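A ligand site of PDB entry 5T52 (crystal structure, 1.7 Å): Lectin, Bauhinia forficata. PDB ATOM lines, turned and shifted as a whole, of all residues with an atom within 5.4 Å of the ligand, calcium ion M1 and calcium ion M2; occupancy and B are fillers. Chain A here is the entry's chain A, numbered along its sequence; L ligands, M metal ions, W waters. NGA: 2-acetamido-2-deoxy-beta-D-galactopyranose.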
ATOM      1  N   GLN A  43     -33.851  -7.992 -25.436  1.00  0.00           N
ATOM      2  CA  GLN A  43     -33.388  -7.081 -24.331  1.00  0.00           C
ATOM      3  C   GLN A  43     -34.606  -6.593 -23.499  1.00  0.00           C
ATOM      4  O   GLN A  43     -34.809  -5.381 -23.357  1.00  0.00           O
ATOM      5  CB  GLN A  43     -32.587  -5.942 -24.872  1.00  0.00           C
ATOM      6  CG  GLN A  43     -31.280  -6.482 -25.451  1.00  0.00           C
ATOM      7  CD  GLN A  43     -30.366  -5.375 -25.990  1.00  0.00           C
ATOM      8  OE1 GLN A  43     -30.801  -4.290 -26.324  1.00  0.00           O
ATOM      9  NE2 GLN A  43     -29.091  -5.649 -26.032  1.00  0.00           N
ATOM     10  N   ALA A  77     -32.123 -17.024 -25.852  1.00  0.00           N
ATOM     11  CA  ALA A  77     -31.555 -16.475 -24.650  1.00  0.00           C
ATOM     12  C   ALA A  77     -32.681 -15.677 -23.988  1.00  0.00           C
ATOM     13  O   ALA A  77     -33.487 -15.061 -24.750  1.00  0.00           O
ATOM     14  CB  ALA A  77     -30.435 -15.554 -24.975  1.00  0.00           C
ATOM     15  N   ASP A  78     -32.723 -15.597 -22.656  1.00  0.00           N
ATOM     16  CA  ASP A  78     -31.686 -15.978 -21.681  1.00  0.00           C
ATOM     17  C   ASP A  78     -32.138 -16.981 -20.712  1.00  0.00           C
ATOM     18  O   ASP A  78     -31.314 -17.585 -20.050  1.00  0.00           O
ATOM     19  CB  ASP A  78     -31.149 -14.762 -20.888  1.00  0.00           C
ATOM     20  CG  ASP A  78     -30.159 -14.007 -21.719  1.00  0.00           C
ATOM     21  OD1 ASP A  78     -28.953 -14.413 -21.687  1.00  0.00           O
ATOM     22  OD2 ASP A  78     -30.521 -13.040 -22.481  1.00  0.00           O
ATOM     23  N   TYR A  94     -32.008  -6.869 -18.084  1.00  0.00           N
ATOM     24  CA  TYR A  94     -32.410  -7.874 -19.083  1.00  0.00           C
ATOM     25  C   TYR A  94     -31.152  -8.700 -19.485  1.00  0.00           C
ATOM     26  O   TYR A  94     -30.075  -8.471 -18.925  1.00  0.00           O
ATOM     27  CB  TYR A  94     -33.118  -7.200 -20.290  1.00  0.00           C
ATOM     28  CG  TYR A  94     -32.342  -6.037 -20.788  1.00  0.00           C
ATOM     29  CD1 TYR A  94     -31.131  -6.232 -21.496  1.00  0.00           C
ATOM     30  CD2 TYR A  94     -32.789  -4.762 -20.592  1.00  0.00           C
ATOM     31  CE1 TYR A  94     -30.411  -5.119 -22.001  1.00  0.00           C
ATOM     32  CE2 TYR A  94     -32.058  -3.699 -21.022  1.00  0.00           C
ATOM     33  CZ  TYR A  94     -30.897  -3.870 -21.767  1.00  0.00           C
ATOM     34  OH  TYR A  94     -30.150  -2.736 -22.187  1.00  0.00           O
ATOM     35  N   GLY A  95     -31.245  -9.588 -20.458  1.00  0.00           N
ATOM     36  CA  GLY A  95     -30.133 -10.354 -20.930  1.00  0.00           C
ATOM     37  C   GLY A  95     -29.746 -11.386 -19.884  1.00  0.00           C
ATOM     38  O   GLY A  95     -30.602 -11.897 -19.169  1.00  0.00           O
ATOM     39  N   GLY A  96     -28.463 -11.673 -19.783  1.00  0.00           N
ATOM     40  CA  GLY A  96     -27.999 -12.755 -18.918  1.00  0.00           C
ATOM     41  C   GLY A  96     -28.134 -12.518 -17.452  1.00  0.00           C
ATOM     42  O   GLY A  96     -28.007 -13.482 -16.656  1.00  0.00           O
ATOM     43  N   TYR A  97     -28.509 -11.276 -17.082  1.00  0.00           N
ATOM     44  CA  TYR A  97     -28.780 -10.962 -15.663  1.00  0.00           C
ATOM     45  C   TYR A  97     -30.173 -11.471 -15.217  1.00  0.00           C
ATOM     46  O   TYR A  97     -30.484 -11.462 -14.003  1.00  0.00           O
ATOM     47  CB  TYR A  97     -28.654  -9.476 -15.442  1.00  0.00           C
ATOM     48  CG  TYR A  97     -27.305  -8.978 -15.809  1.00  0.00           C
ATOM     49  CD1 TYR A  97     -26.196  -9.229 -14.978  1.00  0.00           C
ATOM     50  CD2 TYR A  97     -27.117  -8.249 -16.994  1.00  0.00           C
ATOM     51  CE1 TYR A  97     -24.894  -8.797 -15.348  1.00  0.00           C
ATOM     52  CE2 TYR A  97     -25.887  -7.827 -17.327  1.00  0.00           C
ATOM     53  CZ  TYR A  97     -24.784  -8.086 -16.519  1.00  0.00           C
ATOM     54  OH  TYR A  97     -23.526  -7.588 -16.907  1.00  0.00           O
ATOM     55  N   GLU A 118     -32.606 -20.962 -11.324  1.00  0.00           N
ATOM     56  CA  GLU A 118     -32.584 -20.387 -12.645  1.00  0.00           C
ATOM     57  C   GLU A 118     -32.504 -21.527 -13.737  1.00  0.00           C
ATOM     58  O   GLU A 118     -31.975 -22.625 -13.469  1.00  0.00           O
ATOM     59  CB  GLU A 118     -31.396 -19.419 -12.762  1.00  0.00           C
ATOM     60  CG  GLU A 118     -30.030 -20.138 -12.824  1.00  0.00           C
ATOM     61  CD  GLU A 118     -28.890 -19.295 -13.295  1.00  0.00           C
ATOM     62  OE1 GLU A 118     -28.694 -18.129 -12.867  1.00  0.00           O
ATOM     63  OE2 GLU A 118     -28.089 -19.826 -14.100  1.00  0.00           O
ATOM     64  N   ASP A 120     -31.266 -21.668 -17.396  1.00  0.00           N
ATOM     65  CA  ASP A 120     -30.429 -20.770 -18.133  1.00  0.00           C
ATOM     66  C   ASP A 120     -30.177 -21.307 -19.493  1.00  0.00           C
ATOM     67  O   ASP A 120     -29.473 -22.295 -19.651  1.00  0.00           O
ATOM     68  CB  ASP A 120     -29.060 -20.547 -17.359  1.00  0.00           C
ATOM     69  CG  ASP A 120     -28.145 -19.452 -17.949  1.00  0.00           C
ATOM     70  OD1 ASP A 120     -28.289 -19.107 -19.133  1.00  0.00           O
ATOM     71  OD2 ASP A 120     -27.337 -18.824 -17.169  1.00  0.00           O
ATOM     72  N   TRP A 122     -28.708 -19.604 -22.133  1.00  0.00           N
ATOM     73  CA  TRP A 122     -27.656 -18.900 -22.870  1.00  0.00           C
ATOM     74  C   TRP A 122     -26.356 -18.887 -22.065  1.00  0.00           C
ATOM     75  O   TRP A 122     -26.259 -18.300 -21.018  1.00  0.00           O
ATOM     76  CB  TRP A 122     -28.079 -17.455 -23.236  1.00  0.00           C
ATOM     77  CG  TRP A 122     -27.000 -16.696 -23.916  1.00  0.00           C
ATOM     78  CD1 TRP A 122     -25.979 -15.994 -23.301  1.00  0.00           C
ATOM     79  CD2 TRP A 122     -26.796 -16.577 -25.308  1.00  0.00           C
ATOM     80  NE1 TRP A 122     -25.144 -15.443 -24.274  1.00  0.00           N
ATOM     81  CE2 TRP A 122     -25.671 -15.757 -25.509  1.00  0.00           C
ATOM     82  CE3 TRP A 122     -27.493 -17.063 -26.437  1.00  0.00           C
ATOM     83  CZ2 TRP A 122     -25.173 -15.513 -26.784  1.00  0.00           C
ATOM     84  CZ3 TRP A 122     -27.015 -16.753 -27.673  1.00  0.00           C
ATOM     85  CH2 TRP A 122     -25.905 -15.959 -27.838  1.00  0.00           C
ATOM     86  N   VAL A 123     -25.315 -19.509 -22.614  1.00  0.00           N
ATOM     87  CA  VAL A 123     -24.085 -19.575 -21.895  1.00  0.00           C
ATOM     88  C   VAL A 123     -23.425 -18.174 -22.017  1.00  0.00           C
ATOM     89  O   VAL A 123     -23.020 -17.783 -23.170  1.00  0.00           O
ATOM     90  CB  VAL A 123     -23.159 -20.631 -22.549  1.00  0.00           C
ATOM     91  CG1 VAL A 123     -21.766 -20.555 -21.906  1.00  0.00           C
ATOM     92  CG2 VAL A 123     -23.747 -22.022 -22.324  1.00  0.00           C
ATOM     93  N   ASN A 124     -23.163 -17.533 -20.918  1.00  0.00           N
ATOM     94  CA  ASN A 124     -22.504 -16.240 -20.845  1.00  0.00           C
ATOM     95  C   ASN A 124     -21.032 -16.405 -20.549  1.00  0.00           C
ATOM     96  O   ASN A 124     -20.651 -17.237 -19.740  1.00  0.00           O
ATOM     97  CB  ASN A 124     -23.136 -15.432 -19.714  1.00  0.00           C
ATOM     98  CG  ASN A 124     -24.504 -14.907 -20.082  1.00  0.00           C
ATOM     99  OD1 ASN A 124     -25.552 -15.450 -19.656  1.00  0.00           O
ATOM    100  ND2 ASN A 124     -24.515 -13.765 -20.815  1.00  0.00           N
ATOM    101  N   GLU A 126     -19.367 -13.550 -19.976  1.00  0.00           N
ATOM    102  CA  GLU A 126     -19.092 -12.298 -19.313  1.00  0.00           C
ATOM    103  C   GLU A 126     -18.865 -12.513 -17.804  1.00  0.00           C
ATOM    104  O   GLU A 126     -18.314 -11.628 -17.137  1.00  0.00           O
ATOM    105  CB  GLU A 126     -20.246 -11.296 -19.515  1.00  0.00           C
ATOM    106  CG  GLU A 126     -20.478 -10.911 -21.002  1.00  0.00           C
ATOM    107  CD  GLU A 126     -21.547 -11.701 -21.682  1.00  0.00           C
ATOM    108  OE1 GLU A 126     -21.766 -12.847 -21.316  1.00  0.00           O
ATOM    109  OE2 GLU A 126     -22.180 -11.116 -22.591  1.00  0.00           O
ATOM    110  N   TRP A 127     -19.213 -13.695 -17.331  1.00  0.00           N
ATOM    111  CA  TRP A 127     -18.896 -14.200 -16.000  1.00  0.00           C
ATOM    112  C   TRP A 127     -18.778 -15.692 -16.062  1.00  0.00           C
ATOM    113  O   TRP A 127     -19.043 -16.286 -17.102  1.00  0.00           O
ATOM    114  CB  TRP A 127     -19.967 -13.758 -14.969  1.00  0.00           C
ATOM    115  CG  TRP A 127     -21.392 -14.118 -15.410  1.00  0.00           C
ATOM    116  CD1 TRP A 127     -22.031 -15.341 -15.348  1.00  0.00           C
ATOM    117  CD2 TRP A 127     -22.308 -13.214 -16.042  1.00  0.00           C
ATOM    118  NE1 TRP A 127     -23.271 -15.247 -15.926  1.00  0.00           N
ATOM    119  CE2 TRP A 127     -23.466 -13.946 -16.370  1.00  0.00           C
ATOM    120  CE3 TRP A 127     -22.194 -11.885 -16.469  1.00  0.00           C
ATOM    121  CZ2 TRP A 127     -24.585 -13.354 -16.959  1.00  0.00           C
ATOM    122  CZ3 TRP A 127     -23.352 -11.263 -17.042  1.00  0.00           C
ATOM    123  CH2 TRP A 127     -24.490 -12.049 -17.359  1.00  0.00           C
ATOM    124  N   GLU A 129     -19.751 -19.341 -15.914  1.00  0.00           N
ATOM    125  CA  GLU A 129     -20.806 -20.352 -15.855  1.00  0.00           C
ATOM    126  C   GLU A 129     -20.483 -21.452 -16.766  1.00  0.00           C
ATOM    127  O   GLU A 129     -19.491 -21.375 -17.499  1.00  0.00           O
ATOM    128  CB  GLU A 129     -22.213 -19.794 -16.032  1.00  0.00           C
ATOM    129  CG  GLU A 129     -22.453 -18.959 -17.298  1.00  0.00           C
ATOM    130  CD  GLU A 129     -23.922 -18.393 -17.416  1.00  0.00           C
ATOM    131  OE1 GLU A 129     -24.550 -18.032 -16.398  1.00  0.00           O
ATOM    132  OE2 GLU A 129     -24.438 -18.311 -18.536  1.00  0.00           O
ATOM    133  N   PRO A 130     -21.221 -22.560 -16.646  1.00  0.00           N
ATOM    134  CA  PRO A 130     -20.814 -23.689 -17.446  1.00  0.00           C
ATOM    135  C   PRO A 130     -20.935 -23.514 -18.940  1.00  0.00           C
ATOM    136  O   PRO A 130     -21.637 -22.678 -19.413  1.00  0.00           O
ATOM    137  CB  PRO A 130     -21.773 -24.830 -17.007  1.00  0.00           C
ATOM    138  CG  PRO A 130     -22.467 -24.358 -15.740  1.00  0.00           C
ATOM    139  CD  PRO A 130     -22.384 -22.876 -15.777  1.00  0.00           C
ATOM    140  N   HIS A 134     -27.936 -24.838 -18.481  1.00  0.00           N
ATOM    141  CA  HIS A 134     -27.841 -25.359 -17.140  1.00  0.00           C
ATOM    142  C   HIS A 134     -28.964 -24.838 -16.305  1.00  0.00           C
ATOM    143  O   HIS A 134     -29.512 -23.832 -16.632  1.00  0.00           O
ATOM    144  CB  HIS A 134     -26.438 -25.054 -16.573  1.00  0.00           C
ATOM    145  CG  HIS A 134     -26.064 -23.591 -16.607  1.00  0.00           C
ATOM    146  ND1 HIS A 134     -25.604 -22.994 -17.751  1.00  0.00           N
ATOM    147  CD2 HIS A 134     -26.298 -22.579 -15.732  1.00  0.00           C
ATOM    148  CE1 HIS A 134     -25.423 -21.701 -17.538  1.00  0.00           C
ATOM    149  NE2 HIS A 134     -25.819 -21.417 -16.326  1.00  0.00           N
ATOM    150  N   ILE A 142     -25.245 -13.720  -9.740  1.00  0.00           N
ATOM    151  CA  ILE A 142     -25.554 -14.375 -11.038  1.00  0.00           C
ATOM    152  C   ILE A 142     -24.659 -15.590 -11.366  1.00  0.00           C
ATOM    153  O   ILE A 142     -25.028 -16.476 -12.190  1.00  0.00           O
ATOM    154  CB  ILE A 142     -25.463 -13.354 -12.215  1.00  0.00           C
ATOM    155  CG1 ILE A 142     -26.259 -13.849 -13.468  1.00  0.00           C
ATOM    156  CG2 ILE A 142     -24.012 -13.004 -12.534  1.00  0.00           C
ATOM    157  CD1 ILE A 142     -27.731 -14.223 -13.341  1.00  0.00           C
ATOM    158  N   SER A 144     -23.928 -18.998 -10.224  1.00  0.00           N
ATOM    159  CA  SER A 144     -24.611 -19.958  -9.365  1.00  0.00           C
ATOM    160  C   SER A 144     -23.701 -20.655  -8.423  1.00  0.00           C
ATOM    161  O   SER A 144     -22.595 -21.062  -8.779  1.00  0.00           O
ATOM    162  CB  SER A 144     -25.316 -21.048 -10.210  1.00  0.00           C
ATOM    163  OG  SER A 144     -26.159 -20.485 -11.245  1.00  0.00           O
ATOM    164  N   THR A 210     -35.017 -11.700 -22.016  1.00  0.00           N
ATOM    165  CA  THR A 210     -34.327 -11.849 -23.294  1.00  0.00           C
ATOM    166  C   THR A 210     -33.178 -10.817 -23.362  1.00  0.00           C
ATOM    167  O   THR A 210     -33.203  -9.852 -22.587  1.00  0.00           O
ATOM    168  CB  THR A 210     -35.268 -11.539 -24.466  1.00  0.00           C
ATOM    169  OG1 THR A 210     -35.851 -10.232 -24.282  1.00  0.00           O
ATOM    170  CG2 THR A 210     -36.472 -12.545 -24.501  1.00  0.00           C
ATOM    171  N   GLY A 211     -32.191 -10.994 -24.248  1.00  0.00           N
ATOM    172  CA  GLY A 211     -31.944 -12.157 -25.088  1.00  0.00           C
ATOM    173  C   GLY A 211     -32.530 -12.100 -26.513  1.00  0.00           C
ATOM    174  O   GLY A 211     -32.531 -10.984 -27.153  1.00  0.00           O
ATOM    175  N   GLN A 212     -33.065 -13.212 -26.967  1.00  0.00           N
ATOM    176  CA  GLN A 212     -33.477 -13.317 -28.341  1.00  0.00           C
ATOM    177  C   GLN A 212     -34.158 -14.679 -28.535  1.00  0.00           C
ATOM    178  O   GLN A 212     -33.819 -15.680 -27.861  1.00  0.00           O
ATOM    179  CB  GLN A 212     -32.231 -13.287 -29.302  1.00  0.00           C
ATOM    180  CG  GLN A 212     -31.133 -14.204 -28.875  1.00  0.00           C
ATOM    181  CD  GLN A 212     -29.892 -14.115 -29.750  1.00  0.00           C
ATOM    182  OE1 GLN A 212     -29.392 -12.971 -30.024  1.00  0.00           O
ATOM    183  NE2 GLN A 212     -29.348 -15.250 -30.219  1.00  0.00           N
HETATM  184  C1  NGA L   1     -25.579 -10.638 -24.810  1.00  0.00           C
HETATM  185  C2  NGA L   1     -26.123 -10.936 -23.408  1.00  0.00           C
HETATM  186  C3  NGA L   1     -26.493 -12.389 -23.257  1.00  0.00           C
HETATM  187  C4  NGA L   1     -27.542 -12.748 -24.329  1.00  0.00           C
HETATM  188  C5  NGA L   1     -26.963 -12.266 -25.657  1.00  0.00           C
HETATM  189  C6  NGA L   1     -27.962 -12.494 -26.770  1.00  0.00           C
HETATM  190  C7  NGA L   1     -25.404 -10.038 -21.236  1.00  0.00           C
HETATM  191  C8  NGA L   1     -24.311  -9.713 -20.289  1.00  0.00           C
HETATM  192  N2  NGA L   1     -25.113 -10.592 -22.365  1.00  0.00           N
HETATM  193  O1  NGA L   1     -25.315  -9.278 -24.973  1.00  0.00           O
HETATM  194  O3  NGA L   1     -26.881 -12.731 -21.938  1.00  0.00           O
HETATM  195  O4  NGA L   1     -28.736 -12.033 -24.081  1.00  0.00           O
HETATM  196  O5  NGA L   1     -26.622 -10.899 -25.768  1.00  0.00           O
HETATM  197  O6  NGA L   1     -27.489 -12.082 -28.070  1.00  0.00           O
HETATM  198  O7  NGA L   1     -26.543  -9.749 -20.902  1.00  0.00           O
HETATM  199 CA    CA M   1     -26.654 -17.318 -18.891  1.00  0.00          CA
HETATM  200 CA    CA M   2     -26.229 -19.217 -15.270  1.00  0.00          CA
HETATM  201  O   HOH W   1     -27.907  -7.482 -20.421  1.00  0.00           O
HETATM  202  O   HOH W   2     -29.696  -9.561 -24.497  1.00  0.00           O
HETATM  203  O   HOH W   3     -28.671 -16.284 -19.760  1.00  0.00           O
HETATM  204  O   HOH W   4     -28.364  -8.776 -26.758  1.00  0.00           O
HETATM  205  O   HOH W   5     -26.935 -15.938 -16.946  1.00  0.00           O
HETATM  206  O   HOH W   6     -26.761 -17.104 -14.275  1.00  0.00           O
HETATM  207  O   HOH W   7     -24.974 -19.918 -13.585  1.00  0.00           O
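The side-chain amide nitrogen of Asn 124 sits at hydrogen-bond distance from the side-chain carboxylate of Glu 126, 2.9 Å away.
The backbone NH of Gly 96 sits close to the side-chain carboxylate of Asp 78 (3.4 Å).
The side-chain carboxylate (OD2) of Asp 78 lies close to the backbone NH (N) of Gly 211 (3.2 Å).
N of Gln 212 lies within hydrogen-bond range of O of Ala 77, 2.9 Å away.
The side-chain carboxylate (OE1) of Glu 129 sits close to the indole nitrogen (NE1) of Trp 127.
O of Thr 210 sits at hydrogen-bond distance from N of Gly 95 (2.9 Å).
Merely in contact with the ligand: Gly 211 (3.4 Å), Gly 95 (3.6 Å), Trp 127 (3.7 Å) and Tyr 97 (3.8 Å).
Hydrophobic or aromatic side chains that line the ligand: Tyr 97, Trp 122 and Trp 127.
Ten residues have an atom within 4 Å of the ligand: Asp 78, Gly 95, Gly 96, Tyr 97, Trp 122, Asn 124, Glu 126, Trp 127, Gly 211 and Gln 212.
The nearest printed residue that does not touch the ligand is Ala 77 (4.01 Å).
Of the 22 residues printed, 4 come within 4 Å of calcium ion M2.
The nearest printed residue that does not touch calcium ion M2 is Ser 144 (4.2 Å).
Four residues have an atom within 4 Å of calcium ion M1: Asp 120, Trp 122, Asn 124 and Glu 129.
Along chain A the residues within 4 Å of calcium ion M1 span positions 120 to 129.
The nearest printed residue that does not touch calcium ion M1 is Val 123 (4.5 Å).
O3 of the ligand is in hydrogen-bond range of N of Gly 96 (2.9 Å).
N2 of the ligand is in hydrogen-bond range of OE2 of Glu 126.
An oxygen (O3) of the ligand sits at hydrogen-bond distance from the side-chain amide nitrogen (ND2) of Asn 124, 2.8 Å away.
The side-chain amide oxygen (OE1) of Gln 212 is in hydrogen-bond range of an oxygen (O6) of the ligand (2.9 Å).
OD2 of Asp 78 sits at hydrogen-bond distance from O4 of the ligand (2.6 Å).
Water W6 bridges the side-chain carboxylate (OE1) of Glu 118 (2.6 Å) and the backbone carbonyl oxygen (O) of Ile 142 (2.8 Å).
Water W2 bridges O4 of the ligand and N of Gly 211.
Water W1 bridges an oxygen (O7) of the ligand and the backbone carbonyl oxygen (O) of Tyr 94.
Water W4 bridges O5 of the ligand (2.9 Å) and NE2 of Gln 43 (3.3 Å).
Calcium ion M2 is bound by water W7 (2.2 Å), the side-chain carboxylate (OD2) of Asp 120 (2.2 Å), the side-chain carboxylate (OE2) of Glu 118 (2.3 Å), the side-chain carboxylate (OE1) of Glu 129 (2.3 Å), water W6 (2.4 Å) and a ring nitrogen (NE2) of His 134 (2.5 Å).
Calcium ion M2 has six donor atoms within binding distance.
Calcium ion M1 is bound by the side-chain amide oxygen (OD1) of Asn 124, the backbone carbonyl oxygen (O) of Trp 122, the side-chain carboxylate (OD2) of Asp 120, water W5, water W3, the side-chain carboxylate (OD1) of Asp 120 and the side-chain carboxylate (OE2) of Glu 129.
Calcium ion M1 has seven donor atoms within binding distance.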
